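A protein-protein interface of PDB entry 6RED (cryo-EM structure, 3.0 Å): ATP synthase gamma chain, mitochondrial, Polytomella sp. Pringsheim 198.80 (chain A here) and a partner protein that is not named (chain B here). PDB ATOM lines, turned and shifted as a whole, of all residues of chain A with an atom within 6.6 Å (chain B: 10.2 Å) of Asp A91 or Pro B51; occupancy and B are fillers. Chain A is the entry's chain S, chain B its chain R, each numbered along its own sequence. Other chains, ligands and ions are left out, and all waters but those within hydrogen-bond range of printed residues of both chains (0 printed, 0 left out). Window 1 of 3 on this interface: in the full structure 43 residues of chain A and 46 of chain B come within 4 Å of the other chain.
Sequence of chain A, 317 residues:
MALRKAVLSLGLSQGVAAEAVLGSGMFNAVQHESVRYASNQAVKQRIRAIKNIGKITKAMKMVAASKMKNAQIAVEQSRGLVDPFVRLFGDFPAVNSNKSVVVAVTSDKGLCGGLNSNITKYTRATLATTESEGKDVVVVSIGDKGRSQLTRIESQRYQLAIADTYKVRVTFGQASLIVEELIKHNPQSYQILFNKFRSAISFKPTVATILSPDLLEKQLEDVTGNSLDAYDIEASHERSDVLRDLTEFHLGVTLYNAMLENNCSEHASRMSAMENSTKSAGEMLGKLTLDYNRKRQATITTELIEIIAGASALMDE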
ATOM      1  N   VAL A  82     -27.010  -7.336 -17.548  1.00  0.00           N
ATOM      2  CA  VAL A  82     -26.758  -6.635 -16.292  1.00  0.00           C
ATOM      3  C   VAL A  82     -27.374  -5.253 -16.257  1.00  0.00           C
ATOM      4  O   VAL A  82     -27.614  -4.729 -15.166  1.00  0.00           O
ATOM      5  CB  VAL A  82     -25.256  -6.499 -15.981  1.00  0.00           C
ATOM      6  CG1 VAL A  82     -24.661  -7.840 -15.744  1.00  0.00           C
ATOM      7  CG2 VAL A  82     -24.532  -5.824 -17.102  1.00  0.00           C
ATOM      8  N   ASP A  83     -27.655  -4.654 -17.405  1.00  0.00           N
ATOM      9  CA  ASP A  83     -28.134  -3.280 -17.353  1.00  0.00           C
ATOM     10  C   ASP A  83     -29.644  -3.060 -17.182  1.00  0.00           C
ATOM     11  O   ASP A  83     -29.992  -1.974 -16.720  1.00  0.00           O
ATOM     12  CB  ASP A  83     -27.588  -2.480 -18.547  1.00  0.00           C
ATOM     13  CG  ASP A  83     -27.966  -3.040 -19.886  1.00  0.00           C
ATOM     14  OD1 ASP A  83     -27.054  -3.467 -20.618  1.00  0.00           O
ATOM     15  OD2 ASP A  83     -29.136  -2.915 -20.283  1.00  0.00           O
ATOM     16  N   PHE A  85     -31.291  -4.420 -14.790  1.00  0.00           N
ATOM     17  CA  PHE A  85     -31.439  -4.351 -13.347  1.00  0.00           C
ATOM     18  C   PHE A  85     -30.894  -3.051 -12.790  1.00  0.00           C
ATOM     19  O   PHE A  85     -31.493  -2.470 -11.885  1.00  0.00           O
ATOM     20  CB  PHE A  85     -30.742  -5.521 -12.690  1.00  0.00           C
ATOM     21  CG  PHE A  85     -31.278  -6.844 -13.096  1.00  0.00           C
ATOM     22  CD1 PHE A  85     -32.369  -7.385 -12.456  1.00  0.00           C
ATOM     23  CD2 PHE A  85     -30.682  -7.554 -14.109  1.00  0.00           C
ATOM     24  CE1 PHE A  85     -32.849  -8.599 -12.829  1.00  0.00           C
ATOM     25  CE2 PHE A  85     -31.162  -8.761 -14.481  1.00  0.00           C
ATOM     26  CZ  PHE A  85     -32.240  -9.283 -13.844  1.00  0.00           C
ATOM     27  N   VAL A  86     -29.763  -2.569 -13.310  1.00  0.00           N
ATOM     28  CA  VAL A  86     -29.234  -1.289 -12.859  1.00  0.00           C
ATOM     29  C   VAL A  86     -30.006  -0.133 -13.469  1.00  0.00           C
ATOM     30  O   VAL A  86     -29.906   1.006 -13.003  1.00  0.00           O
ATOM     31  CB  VAL A  86     -27.729  -1.188 -13.178  1.00  0.00           C
ATOM     32  CG1 VAL A  86     -27.497  -0.820 -14.621  1.00  0.00           C
ATOM     33  CG2 VAL A  86     -27.026  -0.242 -12.228  1.00  0.00           C
ATOM     34  N   PHE A  89     -33.174  -1.150 -10.642  1.00  0.00           N
ATOM     35  CA  PHE A  89     -32.818  -0.995  -9.238  1.00  0.00           C
ATOM     36  C   PHE A  89     -31.799   0.100  -8.985  1.00  0.00           C
ATOM     37  O   PHE A  89     -31.682   0.559  -7.849  1.00  0.00           O
ATOM     38  CB  PHE A  89     -32.246  -2.293  -8.691  1.00  0.00           C
ATOM     39  CG  PHE A  89     -33.239  -3.390  -8.571  1.00  0.00           C
ATOM     40  CD1 PHE A  89     -34.566  -3.117  -8.329  1.00  0.00           C
ATOM     41  CD2 PHE A  89     -32.839  -4.704  -8.684  1.00  0.00           C
ATOM     42  CE1 PHE A  89     -35.472  -4.138  -8.204  1.00  0.00           C
ATOM     43  CE2 PHE A  89     -33.735  -5.716  -8.564  1.00  0.00           C
ATOM     44  CZ  PHE A  89     -35.053  -5.436  -8.324  1.00  0.00           C
ATOM     45  N   GLY A  90     -31.040   0.501  -9.982  1.00  0.00           N
ATOM     46  CA  GLY A  90     -30.049   1.524  -9.757  1.00  0.00           C
ATOM     47  C   GLY A  90     -28.742   0.974  -9.212  1.00  0.00           C
ATOM     48  O   GLY A  90     -28.497  -0.232  -9.161  1.00  0.00           O
ATOM     49  N   ASP A  91     -27.894   1.903  -8.787  1.00  0.00           N
ATOM     50  CA  ASP A  91     -26.534   1.606  -8.351  1.00  0.00           C
ATOM     51  C   ASP A  91     -26.310   2.307  -7.022  1.00  0.00           C
ATOM     52  O   ASP A  91     -26.108   3.523  -6.993  1.00  0.00           O
ATOM     53  CB  ASP A  91     -25.519   2.088  -9.380  1.00  0.00           C
ATOM     54  CG  ASP A  91     -24.339   1.174  -9.498  1.00  0.00           C
ATOM     55  OD1 ASP A  91     -23.836   1.021 -10.624  1.00  0.00           O
ATOM     56  OD2 ASP A  91     -23.920   0.592  -8.477  1.00  0.00           O
ATOM     57  N   PHE A  92     -26.335   1.552  -5.926  1.00  0.00           N
ATOM     58  CA  PHE A  92     -26.227   2.108  -4.584  1.00  0.00           C
ATOM     59  C   PHE A  92     -25.053   1.463  -3.857  1.00  0.00           C
ATOM     60  O   PHE A  92     -25.249   0.554  -3.042  1.00  0.00           O
ATOM     61  CB  PHE A  92     -27.526   1.906  -3.812  1.00  0.00           C
ATOM     62  CG  PHE A  92     -28.700   2.610  -4.419  1.00  0.00           C
ATOM     63  CD1 PHE A  92     -28.565   3.885  -4.940  1.00  0.00           C
ATOM     64  CD2 PHE A  92     -29.933   1.994  -4.479  1.00  0.00           C
ATOM     65  CE1 PHE A  92     -29.636   4.528  -5.509  1.00  0.00           C
ATOM     66  CE2 PHE A  92     -31.014   2.637  -5.042  1.00  0.00           C
ATOM     67  CZ  PHE A  92     -30.866   3.903  -5.558  1.00  0.00           C
ATOM     68  N   PRO A  93     -23.822   1.914  -4.118  1.00  0.00           N
ATOM     69  CA  PRO A  93     -22.675   1.302  -3.429  1.00  0.00           C
ATOM     70  C   PRO A  93     -22.549   1.729  -1.986  1.00  0.00           C
ATOM     71  O   PRO A  93     -22.215   0.906  -1.127  1.00  0.00           O
ATOM     72  CB  PRO A  93     -21.477   1.778  -4.262  1.00  0.00           C
ATOM     73  CG  PRO A  93     -22.067   2.362  -5.505  1.00  0.00           C
ATOM     74  CD  PRO A  93     -23.378   2.894  -5.114  1.00  0.00           C
ATOM     75  N   ALA A  94     -22.817   2.993  -1.687  1.00  0.00           N
ATOM     76  CA  ALA A  94     -22.566   3.534  -0.357  1.00  0.00           C
ATOM     77  C   ALA A  94     -23.771   3.398   0.561  1.00  0.00           C
ATOM     78  O   ALA A  94     -24.198   4.360   1.187  1.00  0.00           O
ATOM     79  CB  ALA A  94     -22.142   4.991  -0.478  1.00  0.00           C
ATOM     80  N   PHE A 194     -14.644  -7.123  -9.417  1.00  0.00           N
ATOM     81  CA  PHE A 194     -14.116  -7.809 -10.579  1.00  0.00           C
ATOM     82  C   PHE A 194     -13.451  -6.798 -11.495  1.00  0.00           C
ATOM     83  O   PHE A 194     -13.538  -5.594 -11.281  1.00  0.00           O
ATOM     84  CB  PHE A 194     -15.204  -8.609 -11.303  1.00  0.00           C
ATOM     85  CG  PHE A 194     -16.279  -7.776 -11.940  1.00  0.00           C
ATOM     86  CD1 PHE A 194     -17.374  -7.367 -11.215  1.00  0.00           C
ATOM     87  CD2 PHE A 194     -16.226  -7.464 -13.288  1.00  0.00           C
ATOM     88  CE1 PHE A 194     -18.361  -6.634 -11.803  1.00  0.00           C
ATOM     89  CE2 PHE A 194     -17.213  -6.722 -13.876  1.00  0.00           C
ATOM     90  CZ  PHE A 194     -18.276  -6.308 -13.131  1.00  0.00           C
ATOM     91  N   LYS A 196     -13.450  -5.283 -15.121  1.00  0.00           N
ATOM     92  CA  LYS A 196     -14.244  -5.167 -16.331  1.00  0.00           C
ATOM     93  C   LYS A 196     -13.334  -5.156 -17.548  1.00  0.00           C
ATOM     94  O   LYS A 196     -12.385  -4.378 -17.611  1.00  0.00           O
ATOM     95  CB  LYS A 196     -15.089  -3.901 -16.301  1.00  0.00           C
ATOM     96  CG  LYS A 196     -16.165  -3.859 -17.340  1.00  0.00           C
ATOM     97  CD  LYS A 196     -17.516  -4.116 -16.720  1.00  0.00           C
ATOM     98  CE  LYS A 196     -18.623  -3.910 -17.737  1.00  0.00           C
ATOM     99  NZ  LYS A 196     -19.971  -4.108 -17.147  1.00  0.00           N
ATOM    100  N   THR A 206     -14.050  -2.897 -10.995  1.00  0.00           N
ATOM    101  CA  THR A 206     -15.338  -2.319 -10.651  1.00  0.00           C
ATOM    102  C   THR A 206     -15.890  -2.945  -9.385  1.00  0.00           C
ATOM    103  O   THR A 206     -15.509  -4.053  -9.009  1.00  0.00           O
ATOM    104  CB  THR A 206     -16.374  -2.508 -11.743  1.00  0.00           C
ATOM    105  OG1 THR A 206     -16.937  -3.810 -11.627  1.00  0.00           O
ATOM    106  CG2 THR A 206     -15.749  -2.395 -13.076  1.00  0.00           C
ATOM    107  N   VAL A 207     -16.795  -2.223  -8.740  1.00  0.00           N
ATOM    108  CA  VAL A 207     -17.588  -2.747  -7.642  1.00  0.00           C
ATOM    109  C   VAL A 207     -19.065  -2.608  -8.001  1.00  0.00           C
ATOM    110  O   VAL A 207     -19.528  -1.529  -8.391  1.00  0.00           O
ATOM    111  CB  VAL A 207     -17.228  -2.055  -6.312  1.00  0.00           C
ATOM    112  CG1 VAL A 207     -17.150  -0.557  -6.477  1.00  0.00           C
ATOM    113  CG2 VAL A 207     -18.217  -2.417  -5.239  1.00  0.00           C
ATOM    114  N   ALA A 208     -19.790  -3.719  -7.918  1.00  0.00           N
ATOM    115  CA  ALA A 208     -21.202  -3.778  -8.257  1.00  0.00           C
ATOM    116  C   ALA A 208     -21.962  -4.163  -7.005  1.00  0.00           C
ATOM    117  O   ALA A 208     -21.534  -5.059  -6.276  1.00  0.00           O
ATOM    118  CB  ALA A 208     -21.466  -4.788  -9.369  1.00  0.00           C
ATOM    119  N   THR A 209     -23.081  -3.490  -6.753  1.00  0.00           N
ATOM    120  CA  THR A 209     -23.780  -3.599  -5.482  1.00  0.00           C
ATOM    121  C   THR A 209     -25.208  -4.070  -5.696  1.00  0.00           C
ATOM    122  O   THR A 209     -25.905  -3.568  -6.580  1.00  0.00           O
ATOM    123  CB  THR A 209     -23.765  -2.266  -4.743  1.00  0.00           C
ATOM    124  OG1 THR A 209     -22.482  -1.658  -4.911  1.00  0.00           O
ATOM    125  CG2 THR A 209     -24.003  -2.494  -3.263  1.00  0.00           C
ATOM    126  N   GLU A 221     -35.012   3.208  -2.284  1.00  0.00           N
ATOM    127  CA  GLU A 221     -35.771   3.805  -3.364  1.00  0.00           C
ATOM    128  C   GLU A 221     -36.766   4.834  -2.863  1.00  0.00           C
ATOM    129  O   GLU A 221     -37.422   5.487  -3.679  1.00  0.00           O
ATOM    130  CB  GLU A 221     -36.526   2.724  -4.138  1.00  0.00           C
ATOM    131  CG  GLU A 221     -35.669   1.731  -4.869  1.00  0.00           C
ATOM    132  CD  GLU A 221     -34.978   2.329  -6.054  1.00  0.00           C
ATOM    133  OE1 GLU A 221     -35.520   3.272  -6.659  1.00  0.00           O
ATOM    134  OE2 GLU A 221     -33.892   1.837  -6.395  1.00  0.00           O
ATOM    135  N   HIS A 250     -30.669 -10.876  -9.930  1.00  0.00           N
ATOM    136  CA  HIS A 250     -29.717  -9.811 -10.214  1.00  0.00           C
ATOM    137  C   HIS A 250     -28.347 -10.140  -9.655  1.00  0.00           C
ATOM    138  O   HIS A 250     -27.330  -9.839 -10.286  1.00  0.00           O
ATOM    139  CB  HIS A 250     -30.252  -8.500  -9.653  1.00  0.00           C
ATOM    140  CG  HIS A 250     -29.309  -7.354  -9.779  1.00  0.00           C
ATOM    141  ND1 HIS A 250     -28.512  -7.163 -10.884  1.00  0.00           N
ATOM    142  CD2 HIS A 250     -29.095  -6.290  -8.974  1.00  0.00           C
ATOM    143  CE1 HIS A 250     -27.817  -6.052 -10.734  1.00  0.00           C
ATOM    144  NE2 HIS A 250     -28.154  -5.501  -9.584  1.00  0.00           N
ATOM    145  N   THR A 254     -25.162 -10.577 -12.203  1.00  0.00           N
ATOM    146  CA  THR A 254     -23.929  -9.821 -12.066  1.00  0.00           C
ATOM    147  C   THR A 254     -22.770 -10.705 -11.638  1.00  0.00           C
ATOM    148  O   THR A 254     -21.629 -10.367 -11.928  1.00  0.00           O
ATOM    149  CB  THR A 254     -24.104  -8.662 -11.092  1.00  0.00           C
ATOM    150  OG1 THR A 254     -22.959  -7.807 -11.166  1.00  0.00           O
ATOM    151  CG2 THR A 254     -24.204  -9.162  -9.705  1.00  0.00           C
ATOM    152  N   ALA B  26     -30.145   9.567   3.268  1.00  0.00           N
ATOM    153  CA  ALA B  26     -28.910   8.785   3.206  1.00  0.00           C
ATOM    154  C   ALA B  26     -28.654   8.385   1.760  1.00  0.00           C
ATOM    155  O   ALA B  26     -28.763   7.209   1.397  1.00  0.00           O
ATOM    156  CB  ALA B  26     -28.996   7.555   4.111  1.00  0.00           C
ATOM    157  N   PRO B  27     -28.281   9.339   0.911  1.00  0.00           N
ATOM    158  CA  PRO B  27     -28.275   9.084  -0.534  1.00  0.00           C
ATOM    159  C   PRO B  27     -27.043   8.347  -1.021  1.00  0.00           C
ATOM    160  O   PRO B  27     -26.058   8.981  -1.398  1.00  0.00           O
ATOM    161  CB  PRO B  27     -28.348  10.493  -1.141  1.00  0.00           C
ATOM    162  CG  PRO B  27     -28.195  11.462   0.018  1.00  0.00           C
ATOM    163  CD  PRO B  27     -27.755  10.677   1.211  1.00  0.00           C
ATOM    164  N   ALA B  28     -27.078   7.018  -0.989  1.00  0.00           N
ATOM    165  CA  ALA B  28     -26.047   6.193  -1.606  1.00  0.00           C
ATOM    166  C   ALA B  28     -25.991   6.430  -3.111  1.00  0.00           C
ATOM    167  O   ALA B  28     -26.971   6.833  -3.742  1.00  0.00           O
ATOM    168  CB  ALA B  28     -26.325   4.721  -1.340  1.00  0.00           C
ATOM    169  N   GLY B  29     -24.829   6.180  -3.694  1.00  0.00           N
ATOM    170  CA  GLY B  29     -24.682   6.390  -5.112  1.00  0.00           C
ATOM    171  C   GLY B  29     -23.244   6.399  -5.572  1.00  0.00           C
ATOM    172  O   GLY B  29     -22.314   6.247  -4.779  1.00  0.00           O
ATOM    173  N   PRO B  30     -23.037   6.563  -6.879  1.00  0.00           N
ATOM    174  CA  PRO B  30     -21.667   6.624  -7.406  1.00  0.00           C
ATOM    175  C   PRO B  30     -20.982   7.941  -7.082  1.00  0.00           C
ATOM    176  O   PRO B  30     -19.762   7.989  -6.904  1.00  0.00           O
ATOM    177  CB  PRO B  30     -21.861   6.442  -8.916  1.00  0.00           C
ATOM    178  CG  PRO B  30     -23.233   6.893  -9.182  1.00  0.00           C
ATOM    179  CD  PRO B  30     -24.047   6.627  -7.949  1.00  0.00           C
ATOM    180  N   LYS B  31     -21.756   9.020  -6.998  1.00  0.00           N
ATOM    181  CA  LYS B  31     -21.181  10.296  -6.603  1.00  0.00           C
ATOM    182  C   LYS B  31     -20.922  10.346  -5.104  1.00  0.00           C
ATOM    183  O   LYS B  31     -20.004  11.044  -4.669  1.00  0.00           O
ATOM    184  CB  LYS B  31     -22.106  11.442  -7.042  1.00  0.00           C
ATOM    185  CG  LYS B  31     -21.503  12.851  -6.966  1.00  0.00           C
ATOM    186  CD  LYS B  31     -21.863  13.613  -5.695  1.00  0.00           C
ATOM    187  CE  LYS B  31     -23.298  14.074  -5.703  1.00  0.00           C
ATOM    188  NZ  LYS B  31     -23.636  14.798  -4.448  1.00  0.00           N
ATOM    189  N   GLU B  32     -21.685   9.600  -4.311  1.00  0.00           N
ATOM    190  CA  GLU B  32     -21.594   9.675  -2.862  1.00  0.00           C
ATOM    191  C   GLU B  32     -20.806   8.521  -2.263  1.00  0.00           C
ATOM    192  O   GLU B  32     -20.655   8.454  -1.040  1.00  0.00           O
ATOM    193  CB  GLU B  32     -22.990   9.727  -2.248  1.00  0.00           C
ATOM    194  CG  GLU B  32     -23.780  10.990  -2.569  1.00  0.00           C
ATOM    195  CD  GLU B  32     -24.569  10.894  -3.861  1.00  0.00           C
ATOM    196  OE1 GLU B  32     -24.505   9.844  -4.534  1.00  0.00           O
ATOM    197  OE2 GLU B  32     -25.284  11.864  -4.189  1.00  0.00           O
ATOM    198  N   PHE B  33     -20.330   7.593  -3.089  1.00  0.00           N
ATOM    199  CA  PHE B  33     -19.305   6.653  -2.657  1.00  0.00           C
ATOM    200  C   PHE B  33     -17.920   7.247  -2.824  1.00  0.00           C
ATOM    201  O   PHE B  33     -16.999   6.869  -2.089  1.00  0.00           O
ATOM    202  CB  PHE B  33     -19.420   5.357  -3.460  1.00  0.00           C
ATOM    203  CG  PHE B  33     -18.444   4.290  -3.060  1.00  0.00           C
ATOM    204  CD1 PHE B  33     -17.509   3.822  -3.963  1.00  0.00           C
ATOM    205  CD2 PHE B  33     -18.479   3.742  -1.794  1.00  0.00           C
ATOM    206  CE1 PHE B  33     -16.623   2.839  -3.613  1.00  0.00           C
ATOM    207  CE2 PHE B  33     -17.592   2.755  -1.441  1.00  0.00           C
ATOM    208  CZ  PHE B  33     -16.661   2.305  -2.353  1.00  0.00           C
ATOM    209  N   THR B  34     -17.787   8.200  -3.747  1.00  0.00           N
ATOM    210  CA  THR B  34     -16.489   8.749  -4.106  1.00  0.00           C
ATOM    211  C   THR B  34     -15.876   9.545  -2.962  1.00  0.00           C
ATOM    212  O   THR B  34     -14.670   9.456  -2.734  1.00  0.00           O
ATOM    213  CB  THR B  34     -16.618   9.615  -5.356  1.00  0.00           C
ATOM    214  OG1 THR B  34     -17.389   8.916  -6.341  1.00  0.00           O
ATOM    215  CG2 THR B  34     -15.255   9.930  -5.934  1.00  0.00           C
ATOM    216  N   PRO B  48     -13.004   2.879  -7.908  1.00  0.00           N
ATOM    217  CA  PRO B  48     -13.494   1.727  -8.665  1.00  0.00           C
ATOM    218  C   PRO B  48     -14.745   2.053  -9.448  1.00  0.00           C
ATOM    219  O   PRO B  48     -15.585   2.844  -9.019  1.00  0.00           O
ATOM    220  CB  PRO B  48     -13.788   0.693  -7.577  1.00  0.00           C
ATOM    221  CG  PRO B  48     -13.929   1.476  -6.339  1.00  0.00           C
ATOM    222  CD  PRO B  48     -12.945   2.579  -6.471  1.00  0.00           C
ATOM    223  N   GLU B  49     -14.858   1.432 -10.616  1.00  0.00           N
ATOM    224  CA  GLU B  49     -15.980   1.709 -11.485  1.00  0.00           C
ATOM    225  C   GLU B  49     -17.239   1.025 -10.971  1.00  0.00           C
ATOM    226  O   GLU B  49     -17.226   0.259 -10.007  1.00  0.00           O
ATOM    227  CB  GLU B  49     -15.681   1.262 -12.911  1.00  0.00           C
ATOM    228  CG  GLU B  49     -14.549   1.996 -13.543  1.00  0.00           C
ATOM    229  CD  GLU B  49     -14.861   3.452 -13.732  1.00  0.00           C
ATOM    230  OE1 GLU B  49     -16.024   3.782 -14.040  1.00  0.00           O
ATOM    231  OE2 GLU B  49     -13.947   4.278 -13.543  1.00  0.00           O
ATOM    232  N   PHE B  50     -18.344   1.330 -11.623  1.00  0.00           N
ATOM    233  CA  PHE B  50     -19.670   0.876 -11.248  1.00  0.00           C
ATOM    234  C   PHE B  50     -20.390   0.483 -12.520  1.00  0.00           C
ATOM    235  O   PHE B  50     -20.061   0.983 -13.600  1.00  0.00           O
ATOM    236  CB  PHE B  50     -20.445   1.985 -10.525  1.00  0.00           C
ATOM    237  CG  PHE B  50     -19.689   2.615  -9.408  1.00  0.00           C
ATOM    238  CD1 PHE B  50     -19.056   3.827  -9.588  1.00  0.00           C
ATOM    239  CD2 PHE B  50     -19.603   1.994  -8.178  1.00  0.00           C
ATOM    240  CE1 PHE B  50     -18.358   4.408  -8.571  1.00  0.00           C
ATOM    241  CE2 PHE B  50     -18.903   2.581  -7.152  1.00  0.00           C
ATOM    242  CZ  PHE B  50     -18.285   3.786  -7.352  1.00  0.00           C
ATOM    243  N   PRO B  51     -21.371  -0.418 -12.438  1.00  0.00           N
ATOM    244  CA  PRO B  51     -22.138  -0.753 -13.643  1.00  0.00           C
ATOM    245  C   PRO B  51     -23.014   0.382 -14.143  1.00  0.00           C
ATOM    246  O   PRO B  51     -23.421   0.346 -15.310  1.00  0.00           O
ATOM    247  CB  PRO B  51     -22.972  -1.960 -13.206  1.00  0.00           C
ATOM    248  CG  PRO B  51     -22.964  -1.920 -11.733  1.00  0.00           C
ATOM    249  CD  PRO B  51     -21.666  -1.344 -11.336  1.00  0.00           C
ATOM    250  N   SER B  52     -23.310   1.386 -13.312  1.00  0.00           N
ATOM    251  CA  SER B  52     -24.003   2.575 -13.788  1.00  0.00           C
ATOM    252  C   SER B  52     -23.178   3.380 -14.774  1.00  0.00           C
ATOM    253  O   SER B  52     -23.754   4.100 -15.593  1.00  0.00           O
ATOM    254  CB  SER B  52     -24.376   3.484 -12.628  1.00  0.00           C
ATOM    255  OG  SER B  52     -24.904   4.706 -13.108  1.00  0.00           O
ATOM    256  N   ASN B  53     -21.852   3.292 -14.707  1.00  0.00           N
ATOM    257  CA  ASN B  53     -21.013   4.048 -15.625  1.00  0.00           C
ATOM    258  C   ASN B  53     -21.054   3.478 -17.030  1.00  0.00           C
ATOM    259  O   ASN B  53     -20.783   4.202 -17.992  1.00  0.00           O
ATOM    260  CB  ASN B  53     -19.585   4.076 -15.103  1.00  0.00           C
ATOM    261  CG  ASN B  53     -19.491   4.697 -13.735  1.00  0.00           C
ATOM    262  OD1 ASN B  53     -20.063   5.751 -13.481  1.00  0.00           O
ATOM    263  ND2 ASN B  53     -18.788   4.040 -12.839  1.00  0.00           N
ATOM    264  N   TYR B  54     -21.402   2.204 -17.169  1.00  0.00           N
ATOM    265  CA  TYR B  54     -21.500   1.548 -18.458  1.00  0.00           C
ATOM    266  C   TYR B  54     -22.930   1.460 -18.958  1.00  0.00           C
ATOM    267  O   TYR B  54     -23.200   0.723 -19.909  1.00  0.00           O
ATOM    268  CB  TYR B  54     -20.891   0.154 -18.374  1.00  0.00           C
ATOM    269  CG  TYR B  54     -19.527   0.140 -17.734  1.00  0.00           C
ATOM    270  CD1 TYR B  54     -18.417   0.591 -18.430  1.00  0.00           C
ATOM    271  CD2 TYR B  54     -19.350  -0.325 -16.441  1.00  0.00           C
ATOM    272  CE1 TYR B  54     -17.172   0.583 -17.857  1.00  0.00           C
ATOM    273  CE2 TYR B  54     -18.107  -0.341 -15.859  1.00  0.00           C
ATOM    274  CZ  TYR B  54     -17.022   0.116 -16.573  1.00  0.00           C
ATOM    275  OH  TYR B  54     -15.775   0.109 -16.006  1.00  0.00           O
ATOM    276  N   THR B  55     -23.854   2.192 -18.345  1.00  0.00           N
ATOM    277  CA  THR B  55     -25.261   2.144 -18.713  1.00  0.00           C
ATOM    278  C   THR B  55     -25.653   3.478 -19.331  1.00  0.00           C
ATOM    279  O   THR B  55     -25.648   4.507 -18.648  1.00  0.00           O
ATOM    280  CB  THR B  55     -26.130   1.837 -17.498  1.00  0.00           C
ATOM    281  OG1 THR B  55     -25.557   0.743 -16.779  1.00  0.00           O
ATOM    282  CG2 THR B  55     -27.516   1.443 -17.948  1.00  0.00           C
ATOM    283  N   ALA B  56     -26.005   3.454 -20.613  1.00  0.00           N
ATOM    284  CA  ALA B  56     -26.294   4.672 -21.358  1.00  0.00           C
ATOM    285  C   ALA B  56     -27.750   5.107 -21.261  1.00  0.00           C
ATOM    286  O   ALA B  56     -28.026   6.311 -21.245  1.00  0.00           O
ATOM    287  CB  ALA B  56     -25.921   4.489 -22.830  1.00  0.00           C
ATOM    288  N   VAL B  57     -28.685   4.162 -21.201  1.00  0.00           N
ATOM    289  CA  VAL B  57     -30.109   4.452 -21.117  1.00  0.00           C
ATOM    290  C   VAL B  57     -30.624   4.006 -19.757  1.00  0.00           C
ATOM    291  O   VAL B  57     -30.176   2.991 -19.216  1.00  0.00           O
ATOM    292  CB  VAL B  57     -30.891   3.772 -22.260  1.00  0.00           C
ATOM    293  CG1 VAL B  57     -30.778   4.587 -23.523  1.00  0.00           C
ATOM    294  CG2 VAL B  57     -30.333   2.400 -22.520  1.00  0.00           C
ATOM    295  N   LYS B  58     -31.549   4.774 -19.202  1.00  0.00           N
ATOM    296  CA  LYS B  58     -32.067   4.571 -17.856  1.00  0.00           C
ATOM    297  C   LYS B  58     -33.598   4.527 -17.880  1.00  0.00           C
ATOM    298  O   LYS B  58     -34.221   4.390 -18.932  1.00  0.00           O
ATOM    299  CB  LYS B  58     -31.543   5.654 -16.915  1.00  0.00           C
ATOM    300  CG  LYS B  58     -30.201   5.321 -16.315  1.00  0.00           C
ATOM    301  CD  LYS B  58     -29.732   6.410 -15.379  1.00  0.00           C
ATOM    302  CE  LYS B  58     -28.535   5.953 -14.575  1.00  0.00           C
ATOM    303  NZ  LYS B  58     -27.499   5.333 -15.436  1.00  0.00           N
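The backbone carbonyl oxygen (O) of Glu B49 lies within hydrogen-bond range of the backbone NH (N) of Val A207 (2.8 Å). N of Ser B52 is in hydrogen-bond range of OD1 of Asp A91 (2.8 Å). N of Pro B51 sits close to OD1 of Asp A91 (3.4 Å).
The backbone carbonyl oxygen of Pro B30 is in hydrogen-bond range of the side-chain hydroxyl of Thr B34 (2.6 Å). ND2 of Asn B53 is in hydrogen-bond range of OE1 of Glu B49, at 3.0 Å. The backbone carbonyl oxygen of Pro B51 lies within hydrogen-bond range of the side-chain hydroxyl of Thr B55, 2.6 Å away. The backbone carbonyl oxygen (O) of Phe A194 sits at hydrogen-bond distance from the backbone NH (N) of Thr A206, at 2.8 Å.
CG2 of Thr B55 touches CB of Asp A83 (3.97 Å). Val A86 touches Thr B55 (CG1 to OG1, 3.3 Å). Ala B28 touches Phe A92. Phe B50 touches Pro A93 (CE2 to CG, 3.6 Å). Ala A94 touches Glu B32 (CB to O, 3.8 Å). Phe B33 touches Ala A94. O of Glu B49 touches CA of Thr A206 (3.3 Å). Thr A206 touches Tyr B54 (CG2 to OH, 3.9 Å). Val A207 touches Phe B50 (O to CD2, 3.5 Å). CA of Ala A208 touches CD of Pro B51, at 3.95 Å.
Printed residues of chain B within 4 Å of Asp A83: Thr B55 (3.97 Å). No residue of chain B comes within 4 Å of Gly A90. Of chain B, only Gly B29, Pro B30, Phe B50, Pro B51 and Ser B52 come within 4 Å of Asp A91. Phe A92 touches just one residue of chain B: Ala B28 (3.6 Å). Printed residues of chain B within 4 Å of Pro A93: Gly B29 (3.5 Å) and Phe B50 (3.6 Å). Of the printed residues of chain B, Val A207 touches Pro B48 (3.8 Å), Glu B49 (2.8 Å), Phe B50 (3.5 Å) and Pro B51 (3.6 Å). No residue of chain B comes within 4 Å of Thr A209. Of the printed residues of chain A, Gly B29 touches Asp A91 (3.7 Å) and Pro A93 (3.5 Å). Printed residues of chain A within 4 Å of Phe B50: Asp A91 (3.5 Å), Pro A93 (3.6 Å) and Val A207 (3.5 Å). Pro B51 touches just these residues of chain A: Asp A91 (3.3 Å), Val A207 (3.6 Å) and Ala A208 (3.95 Å). The nearest printed residue of chain A that does not touch Glu B49 is Ala A208 (5.2 Å).
Hydrophobic or aromatic side chains of chain A that line the printed part of chain B: Val A86, Phe A92, Pro A93, Ala A94, Val A207 and Ala A208. Of the 20 printed residues of chain B, 12 touch a printed residue of chain A. Printed residues of chain B that touch a printed residue of chain A: Ala B28, Gly B29, Pro B30, Glu B32, Phe B33, Pro B48, Glu B49, Phe B50, Pro B51, Ser B52, Tyr B54 and Thr B55. Hydrophobic or aromatic side chains of chain B that line the printed part of chain A: Ala B28, Pro B30, Pro B48, Phe B50, Pro B51 and Tyr B54. Along chain B the printed residues that touch a printed residue of chain A span positions 28 to 55. Among the printed residues, no Asp or Glu carboxylate lies within 4 Å of a Lys or Arg side-chain nitrogen of the other chain.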
